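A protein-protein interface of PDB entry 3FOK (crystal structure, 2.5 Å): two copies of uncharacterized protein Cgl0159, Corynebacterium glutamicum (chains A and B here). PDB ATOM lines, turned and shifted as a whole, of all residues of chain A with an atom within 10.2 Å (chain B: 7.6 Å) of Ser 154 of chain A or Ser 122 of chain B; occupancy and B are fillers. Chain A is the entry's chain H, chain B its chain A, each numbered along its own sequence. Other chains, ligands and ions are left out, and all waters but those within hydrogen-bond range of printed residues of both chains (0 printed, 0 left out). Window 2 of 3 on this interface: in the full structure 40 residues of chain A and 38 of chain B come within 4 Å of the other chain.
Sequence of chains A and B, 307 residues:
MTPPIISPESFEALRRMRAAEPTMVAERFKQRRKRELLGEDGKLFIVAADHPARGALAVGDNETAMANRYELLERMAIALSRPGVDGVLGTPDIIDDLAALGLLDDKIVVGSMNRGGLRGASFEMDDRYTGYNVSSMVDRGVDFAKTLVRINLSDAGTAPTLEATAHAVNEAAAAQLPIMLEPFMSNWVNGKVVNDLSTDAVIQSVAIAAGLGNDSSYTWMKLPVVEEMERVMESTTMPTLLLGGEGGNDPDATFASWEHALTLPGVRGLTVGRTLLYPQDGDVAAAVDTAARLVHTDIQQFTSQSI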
ATOM      1  N   SER A 122      19.035  -6.166  13.237  1.00  0.00           N
ATOM      2  CA  SER A 122      19.213  -7.476  12.651  1.00  0.00           C
ATOM      3  C   SER A 122      18.428  -7.515  11.352  1.00  0.00           C
ATOM      4  O   SER A 122      18.693  -8.311  10.451  1.00  0.00           O
ATOM      5  CB  SER A 122      18.695  -8.560  13.607  1.00  0.00           C
ATOM      6  OG  SER A 122      17.311  -8.458  13.809  1.00  0.00           O
ATOM      7  N   MET A 125      18.259  -4.960   6.475  1.00  0.00           N
ATOM      8  CA  MET A 125      18.242  -5.179   5.033  1.00  0.00           C
ATOM      9  C   MET A 125      16.780  -5.131   4.584  1.00  0.00           C
ATOM     10  O   MET A 125      16.479  -4.969   3.402  1.00  0.00           O
ATOM     11  CB  MET A 125      18.869  -6.524   4.657  1.00  0.00           C
ATOM     12  CG  MET A 125      20.384  -6.571   4.798  1.00  0.00           C
ATOM     13  SD  MET A 125      21.270  -4.972   4.115  1.00  0.00           S
ATOM     14  CE  MET A 125      20.686  -5.035   2.275  1.00  0.00           C
ATOM     15  N   ASP A 126      15.879  -5.270   5.553  1.00  0.00           N
ATOM     16  CA  ASP A 126      14.438  -5.221   5.311  1.00  0.00           C
ATOM     17  C   ASP A 126      14.014  -3.763   5.519  1.00  0.00           C
ATOM     18  O   ASP A 126      13.273  -3.434   6.445  1.00  0.00           O
ATOM     19  CB  ASP A 126      13.736  -6.163   6.296  1.00  0.00           C
ATOM     20  CG  ASP A 126      12.222  -6.121   6.188  1.00  0.00           C
ATOM     21  OD1 ASP A 126      11.697  -5.867   5.086  1.00  0.00           O
ATOM     22  OD2 ASP A 126      11.558  -6.364   7.218  1.00  0.00           O
ATOM     23  N   ARG A 150      19.531  -0.946  -0.659  1.00  0.00           N
ATOM     24  CA  ARG A 150      20.706  -1.752  -0.382  1.00  0.00           C
ATOM     25  C   ARG A 150      20.376  -3.191  -0.748  1.00  0.00           C
ATOM     26  O   ARG A 150      19.368  -3.741  -0.314  1.00  0.00           O
ATOM     27  CB  ARG A 150      21.106  -1.630   1.086  1.00  0.00           C
ATOM     28  CG  ARG A 150      21.822  -0.324   1.392  1.00  0.00           C
ATOM     29  CD  ARG A 150      22.030  -0.149   2.879  1.00  0.00           C
ATOM     30  NE  ARG A 150      20.752  -0.046   3.571  1.00  0.00           N
ATOM     31  CZ  ARG A 150      20.616  -0.006   4.891  1.00  0.00           C
ATOM     32  NH1 ARG A 150      21.689  -0.063   5.670  1.00  0.00           N
ATOM     33  NH2 ARG A 150      19.408   0.091   5.432  1.00  0.00           N
ATOM     34  N   ILE A 151      21.237  -3.787  -1.563  1.00  0.00           N
ATOM     35  CA  ILE A 151      21.038  -5.146  -2.036  1.00  0.00           C
ATOM     36  C   ILE A 151      22.021  -6.130  -1.414  1.00  0.00           C
ATOM     37  O   ILE A 151      23.195  -6.169  -1.781  1.00  0.00           O
ATOM     38  CB  ILE A 151      21.172  -5.179  -3.575  1.00  0.00           C
ATOM     39  CG1 ILE A 151      20.187  -4.176  -4.187  1.00  0.00           C
ATOM     40  CG2 ILE A 151      20.935  -6.582  -4.094  1.00  0.00           C
ATOM     41  CD1 ILE A 151      20.354  -3.950  -5.668  1.00  0.00           C
ATOM     42  N   ASN A 152      21.531  -6.925  -0.468  1.00  0.00           N
ATOM     43  CA  ASN A 152      22.359  -7.918   0.207  1.00  0.00           C
ATOM     44  C   ASN A 152      21.950  -9.313  -0.256  1.00  0.00           C
ATOM     45  O   ASN A 152      20.938  -9.858   0.183  1.00  0.00           O
ATOM     46  CB  ASN A 152      22.196  -7.786   1.722  1.00  0.00           C
ATOM     47  CG  ASN A 152      23.204  -8.608   2.498  1.00  0.00           C
ATOM     48  OD1 ASN A 152      23.657  -8.200   3.570  1.00  0.00           O
ATOM     49  ND2 ASN A 152      23.553  -9.776   1.972  1.00  0.00           N
ATOM     50  N   LEU A 153      22.756  -9.884  -1.143  1.00  0.00           N
ATOM     51  CA  LEU A 153      22.487 -11.199  -1.708  1.00  0.00           C
ATOM     52  C   LEU A 153      22.277 -12.351  -0.731  1.00  0.00           C
ATOM     53  O   LEU A 153      21.613 -13.329  -1.072  1.00  0.00           O
ATOM     54  CB  LEU A 153      23.596 -11.571  -2.694  1.00  0.00           C
ATOM     55  CG  LEU A 153      23.711 -10.656  -3.918  1.00  0.00           C
ATOM     56  CD1 LEU A 153      24.838 -11.144  -4.821  1.00  0.00           C
ATOM     57  CD2 LEU A 153      22.391 -10.638  -4.671  1.00  0.00           C
ATOM     58  N   SER A 154      22.817 -12.249   0.479  1.00  0.00           N
ATOM     59  CA  SER A 154      22.657 -13.336   1.435  1.00  0.00           C
ATOM     60  C   SER A 154      21.580 -13.069   2.478  1.00  0.00           C
ATOM     61  O   SER A 154      21.392 -13.862   3.399  1.00  0.00           O
ATOM     62  CB  SER A 154      23.979 -13.617   2.147  1.00  0.00           C
ATOM     63  OG  SER A 154      24.270 -12.587   3.071  1.00  0.00           O
ATOM     64  N   ASP A 155      20.865 -11.960   2.330  1.00  0.00           N
ATOM     65  CA  ASP A 155      19.826 -11.601   3.289  1.00  0.00           C
ATOM     66  C   ASP A 155      18.440 -11.520   2.641  1.00  0.00           C
ATOM     67  O   ASP A 155      18.183 -10.650   1.811  1.00  0.00           O
ATOM     68  CB  ASP A 155      20.178 -10.259   3.934  1.00  0.00           C
ATOM     69  CG  ASP A 155      19.366  -9.980   5.176  1.00  0.00           C
ATOM     70  OD1 ASP A 155      18.128 -10.121   5.119  1.00  0.00           O
ATOM     71  OD2 ASP A 155      19.962  -9.614   6.210  1.00  0.00           O
ATOM     72  N   ALA A 156      17.549 -12.420   3.040  1.00  0.00           N
ATOM     73  CA  ALA A 156      16.194 -12.474   2.499  1.00  0.00           C
ATOM     74  C   ALA A 156      15.436 -11.153   2.593  1.00  0.00           C
ATOM     75  O   ALA A 156      14.487 -10.920   1.839  1.00  0.00           O
ATOM     76  CB  ALA A 156      15.400 -13.574   3.194  1.00  0.00           C
ATOM     77  N   GLY A 157      15.850 -10.295   3.520  1.00  0.00           N
ATOM     78  CA  GLY A 157      15.190  -9.013   3.682  1.00  0.00           C
ATOM     79  C   GLY A 157      15.280  -8.148   2.439  1.00  0.00           C
ATOM     80  O   GLY A 157      14.460  -7.252   2.239  1.00  0.00           O
ATOM     81  N   THR A 158      16.281  -8.408   1.606  1.00  0.00           N
ATOM     82  CA  THR A 158      16.461  -7.641   0.383  1.00  0.00           C
ATOM     83  C   THR A 158      15.272  -7.835  -0.548  1.00  0.00           C
ATOM     84  O   THR A 158      14.842  -6.900  -1.219  1.00  0.00           O
ATOM     85  CB  THR A 158      17.739  -8.072  -0.370  1.00  0.00           C
ATOM     86  OG1 THR A 158      18.889  -7.817   0.446  1.00  0.00           O
ATOM     87  CG2 THR A 158      17.871  -7.297  -1.682  1.00  0.00           C
ATOM     88  N   ALA A 159      14.748  -9.058  -0.585  1.00  0.00           N
ATOM     89  CA  ALA A 159      13.617  -9.386  -1.446  1.00  0.00           C
ATOM     90  C   ALA A 159      12.440  -8.417  -1.293  1.00  0.00           C
ATOM     91  O   ALA A 159      12.062  -7.738  -2.250  1.00  0.00           O
ATOM     92  CB  ALA A 159      13.164 -10.818  -1.191  1.00  0.00           C
ATOM     93  N   PRO A 160      11.840  -8.335  -0.094  1.00  0.00           N
ATOM     94  CA  PRO A 160      10.721  -7.395   0.006  1.00  0.00           C
ATOM     95  C   PRO A 160      11.096  -5.936  -0.271  1.00  0.00           C
ATOM     96  O   PRO A 160      10.238  -5.138  -0.665  1.00  0.00           O
ATOM     97  CB  PRO A 160      10.195  -7.624   1.424  1.00  0.00           C
ATOM     98  CG  PRO A 160      11.392  -8.142   2.167  1.00  0.00           C
ATOM     99  CD  PRO A 160      12.022  -9.075   1.168  1.00  0.00           C
ATOM    100  N   LEU A 162      13.278  -4.919  -2.607  1.00  0.00           N
ATOM    101  CA  LEU A 162      13.337  -4.740  -4.050  1.00  0.00           C
ATOM    102  C   LEU A 162      11.919  -4.527  -4.577  1.00  0.00           C
ATOM    103  O   LEU A 162      11.672  -3.626  -5.377  1.00  0.00           O
ATOM    104  CB  LEU A 162      13.955  -5.968  -4.719  1.00  0.00           C
ATOM    105  CG  LEU A 162      15.439  -6.230  -4.452  1.00  0.00           C
ATOM    106  CD1 LEU A 162      15.843  -7.563  -5.066  1.00  0.00           C
ATOM    107  CD2 LEU A 162      16.273  -5.103  -5.036  1.00  0.00           C
ATOM    108  N   MET A 185      25.500  -2.569  -3.026  1.00  0.00           N
ATOM    109  CA  MET A 185      25.574  -4.009  -2.870  1.00  0.00           C
ATOM    110  C   MET A 185      26.058  -4.010  -1.422  1.00  0.00           C
ATOM    111  O   MET A 185      26.964  -3.251  -1.081  1.00  0.00           O
ATOM    112  CB  MET A 185      26.632  -4.626  -3.786  1.00  0.00           C
ATOM    113  CG  MET A 185      26.305  -4.571  -5.272  1.00  0.00           C
ATOM    114  SD  MET A 185      24.720  -5.578  -5.779  1.00  0.00           S
ATOM    115  CE  MET A 185      23.428  -4.206  -5.485  1.00  0.00           C
ATOM    116  N   SER A 186      25.439  -4.806  -0.563  1.00  0.00           N
ATOM    117  CA  SER A 186      25.845  -4.837   0.834  1.00  0.00           C
ATOM    118  C   SER A 186      26.065  -6.250   1.336  1.00  0.00           C
ATOM    119  O   SER A 186      25.447  -7.192   0.843  1.00  0.00           O
ATOM    120  CB  SER A 186      24.790  -4.146   1.702  1.00  0.00           C
ATOM    121  OG  SER A 186      24.620  -2.790   1.321  1.00  0.00           O
ATOM    122  N   ASN A 187      26.947  -6.391   2.319  1.00  0.00           N
ATOM    123  CA  ASN A 187      27.239  -7.697   2.886  1.00  0.00           C
ATOM    124  C   ASN A 187      27.299  -7.624   4.397  1.00  0.00           C
ATOM    125  O   ASN A 187      27.539  -6.561   4.969  1.00  0.00           O
ATOM    126  CB  ASN A 187      28.585  -8.230   2.385  1.00  0.00           C
ATOM    127  CG  ASN A 187      28.676  -8.278   0.880  1.00  0.00           C
ATOM    128  OD1 ASN A 187      29.086  -7.312   0.243  1.00  0.00           O
ATOM    129  ND2 ASN A 187      28.293  -9.405   0.303  1.00  0.00           N
ATOM    130  N   TRP A 188      27.073  -8.763   5.039  1.00  0.00           N
ATOM    131  CA  TRP A 188      27.163  -8.835   6.483  1.00  0.00           C
ATOM    132  C   TRP A 188      28.610  -9.198   6.768  1.00  0.00           C
ATOM    133  O   TRP A 188      29.106 -10.214   6.285  1.00  0.00           O
ATOM    134  CB  TRP A 188      26.244  -9.921   7.042  1.00  0.00           C
ATOM    135  CG  TRP A 188      24.808  -9.514   7.141  1.00  0.00           C
ATOM    136  CD1 TRP A 188      23.785  -9.907   6.329  1.00  0.00           C
ATOM    137  CD2 TRP A 188      24.232  -8.636   8.115  1.00  0.00           C
ATOM    138  NE1 TRP A 188      22.606  -9.328   6.736  1.00  0.00           N
ATOM    139  CE2 TRP A 188      22.853  -8.539   7.828  1.00  0.00           C
ATOM    140  CE3 TRP A 188      24.749  -7.913   9.199  1.00  0.00           C
ATOM    141  CZ2 TRP A 188      21.982  -7.757   8.590  1.00  0.00           C
ATOM    142  CZ3 TRP A 188      23.881  -7.131   9.959  1.00  0.00           C
ATOM    143  CH2 TRP A 188      22.514  -7.057   9.646  1.00  0.00           C
ATOM    144  N   VAL A 189      29.293  -8.350   7.528  1.00  0.00           N
ATOM    145  CA  VAL A 189      30.687  -8.585   7.879  1.00  0.00           C
ATOM    146  C   VAL A 189      30.868  -8.333   9.370  1.00  0.00           C
ATOM    147  O   VAL A 189      30.778  -7.194   9.829  1.00  0.00           O
ATOM    148  CB  VAL A 189      31.627  -7.649   7.093  1.00  0.00           C
ATOM    149  CG1 VAL A 189      33.074  -7.917   7.481  1.00  0.00           C
ATOM    150  CG2 VAL A 189      31.432  -7.855   5.604  1.00  0.00           C
ATOM    151  N   LYS A 192      27.865  -6.746  11.057  1.00  0.00           N
ATOM    152  CA  LYS A 192      27.493  -5.396  10.646  1.00  0.00           C
ATOM    153  C   LYS A 192      27.339  -5.324   9.135  1.00  0.00           C
ATOM    154  O   LYS A 192      27.945  -6.102   8.400  1.00  0.00           O
ATOM    155  CB  LYS A 192      28.547  -4.378  11.104  1.00  0.00           C
ATOM    156  CG  LYS A 192      28.823  -4.388  12.598  1.00  0.00           C
ATOM    157  CD  LYS A 192      29.795  -3.288  12.986  1.00  0.00           C
ATOM    158  CE  LYS A 192      30.318  -3.479  14.404  1.00  0.00           C
ATOM    159  NZ  LYS A 192      31.132  -4.724  14.526  1.00  0.00           N
ATOM    160  N   VAL A 193      26.523  -4.382   8.675  1.00  0.00           N
ATOM    161  CA  VAL A 193      26.297  -4.205   7.247  1.00  0.00           C
ATOM    162  C   VAL A 193      27.331  -3.250   6.658  1.00  0.00           C
ATOM    163  O   VAL A 193      27.463  -2.120   7.115  1.00  0.00           O
ATOM    164  CB  VAL A 193      24.889  -3.624   6.970  1.00  0.00           C
ATOM    165  CG1 VAL A 193      24.721  -3.352   5.482  1.00  0.00           C
ATOM    166  CG2 VAL A 193      23.820  -4.591   7.460  1.00  0.00           C
ATOM    167  N   VAL A 194      28.076  -3.714   5.662  1.00  0.00           N
ATOM    168  CA  VAL A 194      29.069  -2.873   5.009  1.00  0.00           C
ATOM    169  C   VAL A 194      28.778  -2.818   3.514  1.00  0.00           C
ATOM    170  O   VAL A 194      28.634  -3.852   2.861  1.00  0.00           O
ATOM    171  CB  VAL A 194      30.515  -3.397   5.222  1.00  0.00           C
ATOM    172  CG1 VAL A 194      30.834  -3.460   6.701  1.00  0.00           C
ATOM    173  CG2 VAL A 194      30.685  -4.757   4.577  1.00  0.00           C
ATOM    174  N   LEU B 118      17.483 -12.349  -7.854  1.00  0.00           N
ATOM    175  CA  LEU B 118      18.817 -11.944  -8.284  1.00  0.00           C
ATOM    176  C   LEU B 118      19.824 -13.088  -8.346  1.00  0.00           C
ATOM    177  O   LEU B 118      19.816 -13.997  -7.514  1.00  0.00           O
ATOM    178  CB  LEU B 118      19.351 -10.853  -7.356  1.00  0.00           C
ATOM    179  CG  LEU B 118      18.530  -9.565  -7.290  1.00  0.00           C
ATOM    180  CD1 LEU B 118      19.172  -8.608  -6.293  1.00  0.00           C
ATOM    181  CD2 LEU B 118      18.444  -8.926  -8.669  1.00  0.00           C
ATOM    182  N   ARG B 119      20.701 -13.031  -9.339  1.00  0.00           N
ATOM    183  CA  ARG B 119      21.719 -14.053  -9.498  1.00  0.00           C
ATOM    184  C   ARG B 119      22.628 -14.088  -8.271  1.00  0.00           C
ATOM    185  O   ARG B 119      23.136 -13.052  -7.835  1.00  0.00           O
ATOM    186  CB  ARG B 119      22.564 -13.766 -10.737  1.00  0.00           C
ATOM    187  CG  ARG B 119      23.578 -14.847 -11.022  1.00  0.00           C
ATOM    188  CD  ARG B 119      24.594 -14.394 -12.051  1.00  0.00           C
ATOM    189  NE  ARG B 119      25.447 -15.499 -12.466  1.00  0.00           N
ATOM    190  CZ  ARG B 119      26.748 -15.380 -12.706  1.00  0.00           C
ATOM    191  NH1 ARG B 119      27.346 -14.201 -12.567  1.00  0.00           N
ATOM    192  NH2 ARG B 119      27.454 -16.437 -13.089  1.00  0.00           N
ATOM    193  N   GLY B 120      22.822 -15.282  -7.716  1.00  0.00           N
ATOM    194  CA  GLY B 120      23.680 -15.433  -6.556  1.00  0.00           C
ATOM    195  C   GLY B 120      23.045 -15.117  -5.215  1.00  0.00           C
ATOM    196  O   GLY B 120      23.714 -15.177  -4.185  1.00  0.00           O
ATOM    197  N   ALA B 121      21.760 -14.786  -5.212  1.00  0.00           N
ATOM    198  CA  ALA B 121      21.071 -14.461  -3.969  1.00  0.00           C
ATOM    199  C   ALA B 121      20.589 -15.713  -3.252  1.00  0.00           C
ATOM    200  O   ALA B 121      20.243 -16.708  -3.882  1.00  0.00           O
ATOM    201  CB  ALA B 121      19.888 -13.544  -4.260  1.00  0.00           C
ATOM    202  N   SER B 122      20.570 -15.666  -1.927  1.00  0.00           N
ATOM    203  CA  SER B 122      20.101 -16.805  -1.151  1.00  0.00           C
ATOM    204  C   SER B 122      18.603 -16.926  -1.407  1.00  0.00           C
ATOM    205  O   SER B 122      18.002 -17.979  -1.205  1.00  0.00           O
ATOM    206  CB  SER B 122      20.352 -16.576   0.341  1.00  0.00           C
ATOM    207  OG  SER B 122      19.616 -15.463   0.815  1.00  0.00           O
ATOM    208  N   PHE B 123      18.018 -15.829  -1.873  1.00  0.00           N
ATOM    209  CA  PHE B 123      16.596 -15.761  -2.156  1.00  0.00           C
ATOM    210  C   PHE B 123      16.258 -15.728  -3.642  1.00  0.00           C
ATOM    211  O   PHE B 123      15.173 -15.268  -4.002  1.00  0.00           O
ATOM    212  CB  PHE B 123      16.016 -14.506  -1.490  1.00  0.00           C
ATOM    213  CG  PHE B 123      16.674 -13.216  -1.936  1.00  0.00           C
ATOM    214  CD1 PHE B 123      16.318 -12.612  -3.141  1.00  0.00           C
ATOM    215  CD2 PHE B 123      17.667 -12.623  -1.161  1.00  0.00           C
ATOM    216  CE1 PHE B 123      16.944 -11.433  -3.568  1.00  0.00           C
ATOM    217  CE2 PHE B 123      18.297 -11.450  -1.576  1.00  0.00           C
ATOM    218  CZ  PHE B 123      17.936 -10.856  -2.780  1.00  0.00           C
ATOM    219  N   GLU B 124      17.137 -16.212  -4.520  1.00  0.00           N
ATOM    220  CA  GLU B 124      16.790 -16.106  -5.935  1.00  0.00           C
ATOM    221  C   GLU B 124      15.676 -17.009  -6.450  1.00  0.00           C
ATOM    222  O   GLU B 124      15.267 -16.882  -7.602  1.00  0.00           O
ATOM    223  CB  GLU B 124      18.037 -16.185  -6.842  1.00  0.00           C
ATOM    224  CG  GLU B 124      18.648 -17.536  -7.148  1.00  0.00           C
ATOM    225  CD  GLU B 124      19.784 -17.401  -8.165  1.00  0.00           C
ATOM    226  OE1 GLU B 124      19.504 -17.084  -9.344  1.00  0.00           O
ATOM    227  OE2 GLU B 124      20.959 -17.591  -7.782  1.00  0.00           O
ATOM    228  N   MET B 125      15.167 -17.910  -5.615  1.00  0.00           N
ATOM    229  CA  MET B 125      14.056 -18.746  -6.050  1.00  0.00           C
ATOM    230  C   MET B 125      12.769 -17.958  -5.795  1.00  0.00           C
ATOM    231  O   MET B 125      11.712 -18.272  -6.340  1.00  0.00           O
ATOM    232  CB  MET B 125      14.023 -20.078  -5.295  1.00  0.00           C
ATOM    233  CG  MET B 125      15.114 -21.054  -5.708  1.00  0.00           C
ATOM    234  SD  MET B 125      15.395 -21.142  -7.626  1.00  0.00           S
ATOM    235  CE  MET B 125      13.624 -21.719  -8.184  1.00  0.00           C
ATOM    236  N   ASP B 126      12.882 -16.927  -4.961  1.00  0.00           N
ATOM    237  CA  ASP B 126      11.766 -16.048  -4.619  1.00  0.00           C
ATOM    238  C   ASP B 126      11.826 -14.878  -5.604  1.00  0.00           C
ATOM    239  O   ASP B 126      12.061 -13.733  -5.229  1.00  0.00           O
ATOM    240  CB  ASP B 126      11.924 -15.574  -3.167  1.00  0.00           C
ATOM    241  CG  ASP B 126      10.856 -14.586  -2.744  1.00  0.00           C
ATOM    242  OD1 ASP B 126       9.722 -14.653  -3.261  1.00  0.00           O
ATOM    243  OD2 ASP B 126      11.154 -13.749  -1.872  1.00  0.00           O
ATOM    244  N   ASP B 155      12.928 -25.513  -2.428  1.00  0.00           N
ATOM    245  CA  ASP B 155      13.004 -24.129  -1.963  1.00  0.00           C
ATOM    246  C   ASP B 155      11.625 -23.473  -1.850  1.00  0.00           C
ATOM    247  O   ASP B 155      10.952 -23.244  -2.850  1.00  0.00           O
ATOM    248  CB  ASP B 155      13.887 -23.324  -2.917  1.00  0.00           C
ATOM    249  CG  ASP B 155      14.315 -22.000  -2.335  1.00  0.00           C
ATOM    250  OD1 ASP B 155      13.445 -21.269  -1.823  1.00  0.00           O
ATOM    251  OD2 ASP B 155      15.523 -21.685  -2.400  1.00  0.00           O
ATOM    252  N   TRP B 188      19.410 -26.631  -6.004  1.00  0.00           N
ATOM    253  CA  TRP B 188      20.535 -25.996  -5.348  1.00  0.00           C
ATOM    254  C   TRP B 188      21.653 -27.024  -5.406  1.00  0.00           C
ATOM    255  O   TRP B 188      21.491 -28.151  -4.925  1.00  0.00           O
ATOM    256  CB  TRP B 188      20.215 -25.670  -3.888  1.00  0.00           C
ATOM    257  CG  TRP B 188      19.399 -24.432  -3.700  1.00  0.00           C
ATOM    258  CD1 TRP B 188      18.077 -24.364  -3.379  1.00  0.00           C
ATOM    259  CD2 TRP B 188      19.854 -23.082  -3.826  1.00  0.00           C
ATOM    260  NE1 TRP B 188      17.680 -23.051  -3.291  1.00  0.00           N
ATOM    261  CE2 TRP B 188      18.752 -22.243  -3.560  1.00  0.00           C
ATOM    262  CE3 TRP B 188      21.090 -22.498  -4.131  1.00  0.00           C
ATOM    263  CZ2 TRP B 188      18.842 -20.848  -3.596  1.00  0.00           C
ATOM    264  CZ3 TRP B 188      21.184 -21.107  -4.167  1.00  0.00           C
ATOM    265  CH2 TRP B 188      20.064 -20.299  -3.896  1.00  0.00           C
ATOM    266  N   GLY B 191      25.558 -24.694  -3.305  1.00  0.00           N
ATOM    267  CA  GLY B 191      25.218 -23.317  -3.000  1.00  0.00           C
ATOM    268  C   GLY B 191      24.838 -22.444  -4.182  1.00  0.00           C
ATOM    269  O   GLY B 191      24.716 -21.224  -4.034  1.00  0.00           O
ATOM    270  N   VAL B 193      22.297 -22.084  -7.914  1.00  0.00           N
ATOM    271  CA  VAL B 193      21.107 -22.560  -8.602  1.00  0.00           C
ATOM    272  C   VAL B 193      21.465 -23.047 -10.000  1.00  0.00           C
ATOM    273  O   VAL B 193      22.024 -22.292 -10.800  1.00  0.00           O
ATOM    274  CB  VAL B 193      20.051 -21.437  -8.733  1.00  0.00           C
ATOM    275  CG1 VAL B 193      18.863 -21.934  -9.548  1.00  0.00           C
ATOM    276  CG2 VAL B 193      19.602 -20.981  -7.355  1.00  0.00           C
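Positions printed for both chains: 122, 125, 126, 155, 188 and 193.
N of Gly 157 of chain A is in hydrogen-bond range of OD1 of Asp 155 of chain A, 2.8 Å away. The side-chain amide nitrogen (ND2) of Asn 152 of chain A lies close to the backbone carbonyl oxygen (O) of Ser 186 of chain A (3.4 Å). The indole nitrogen (NE1) of Trp 188 of chain A sits at hydrogen-bond distance from the side-chain carboxylate (OD2) of Asp 155 of chain A, 2.7 Å away. ND2 of Asn 152 of chain A sits close to N of Ser 154 of chain A. The backbone carbonyl oxygen of Asn 152 of chain A is in hydrogen-bond range of the side-chain hydroxyl of Thr 158 of chain A, at 2.9 Å. The backbone NH (N) of Gly 120 of chain B is in hydrogen-bond range of the side-chain carboxylate (OE2) of Glu 124 of chain B.
Printed residues of chain B within 4 Å of Leu 153 of chain A: Arg 119 (3.95 Å), Gly 120 (3.9 Å), Ala 121 (3.2 Å), Ser 122 (2.7 Å) and Phe 123 (3.8 Å). Printed residues of chain B within 4 Å of Ser 154 of chain A: Ser 122 (3.5 Å). Printed residues of chain B within 4 Å of Leu 162 of chain A: Leu 118 (3.7 Å). Printed residues of chain A within 4 Å of Leu 118 of chain B: Ile 151 and Leu 162. Of the printed residues of chain A, Ser 122 of chain B touches Leu 153 and Ser 154. The nearest residue of chain B that does not touch Ser 154 of chain A is Phe 123 of chain B (5.0 Å).
N of Ser 122 of chain B sits at hydrogen-bond distance from O of Leu 153 of chain A (2.7 Å).
Hydrophobic or aromatic side chains of chain A that line the printed part of chain B: Ile 151, Leu 153, Ala 159 and Leu 162. Of the 13 printed residues of chain B, 7 touch a printed residue of chain A. Among the printed residues, 13 pairs touch across the chains. Among the printed residues, no Asp or Glu carboxylate lies within 4 Å of a Lys or Arg side-chain nitrogen of the other chain.
CG2 of Ile 151 of chain A touches CD1 of Leu 118 of chain B (3.5 Å). CE2 of Phe 123 of chain B touches O of Asn 152 of chain A, 3.6 Å away. O of Gly 120 of chain B touches CB of Leu 153 of chain A, 3.9 Å away. Leu 153 of chain A touches Ala 121 of chain B. Leu 153 of chain A touches Phe 123 of chain B. Ser 122 of chain B touches Ser 154 of chain A. CE2 of Phe 123 of chain B touches O of Asp 155 of chain A, 3.5 Å away. Ala 156 of chain A touches Phe 123 of chain B (CA to CD2, 3.9 Å). CB of Thr 158 of chain A touches CE2 of Phe 123 of chain B, at 3.6 Å. CB of Ala 159 of chain A touches OD2 of Asp 126 of chain B, at 3.6 Å.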
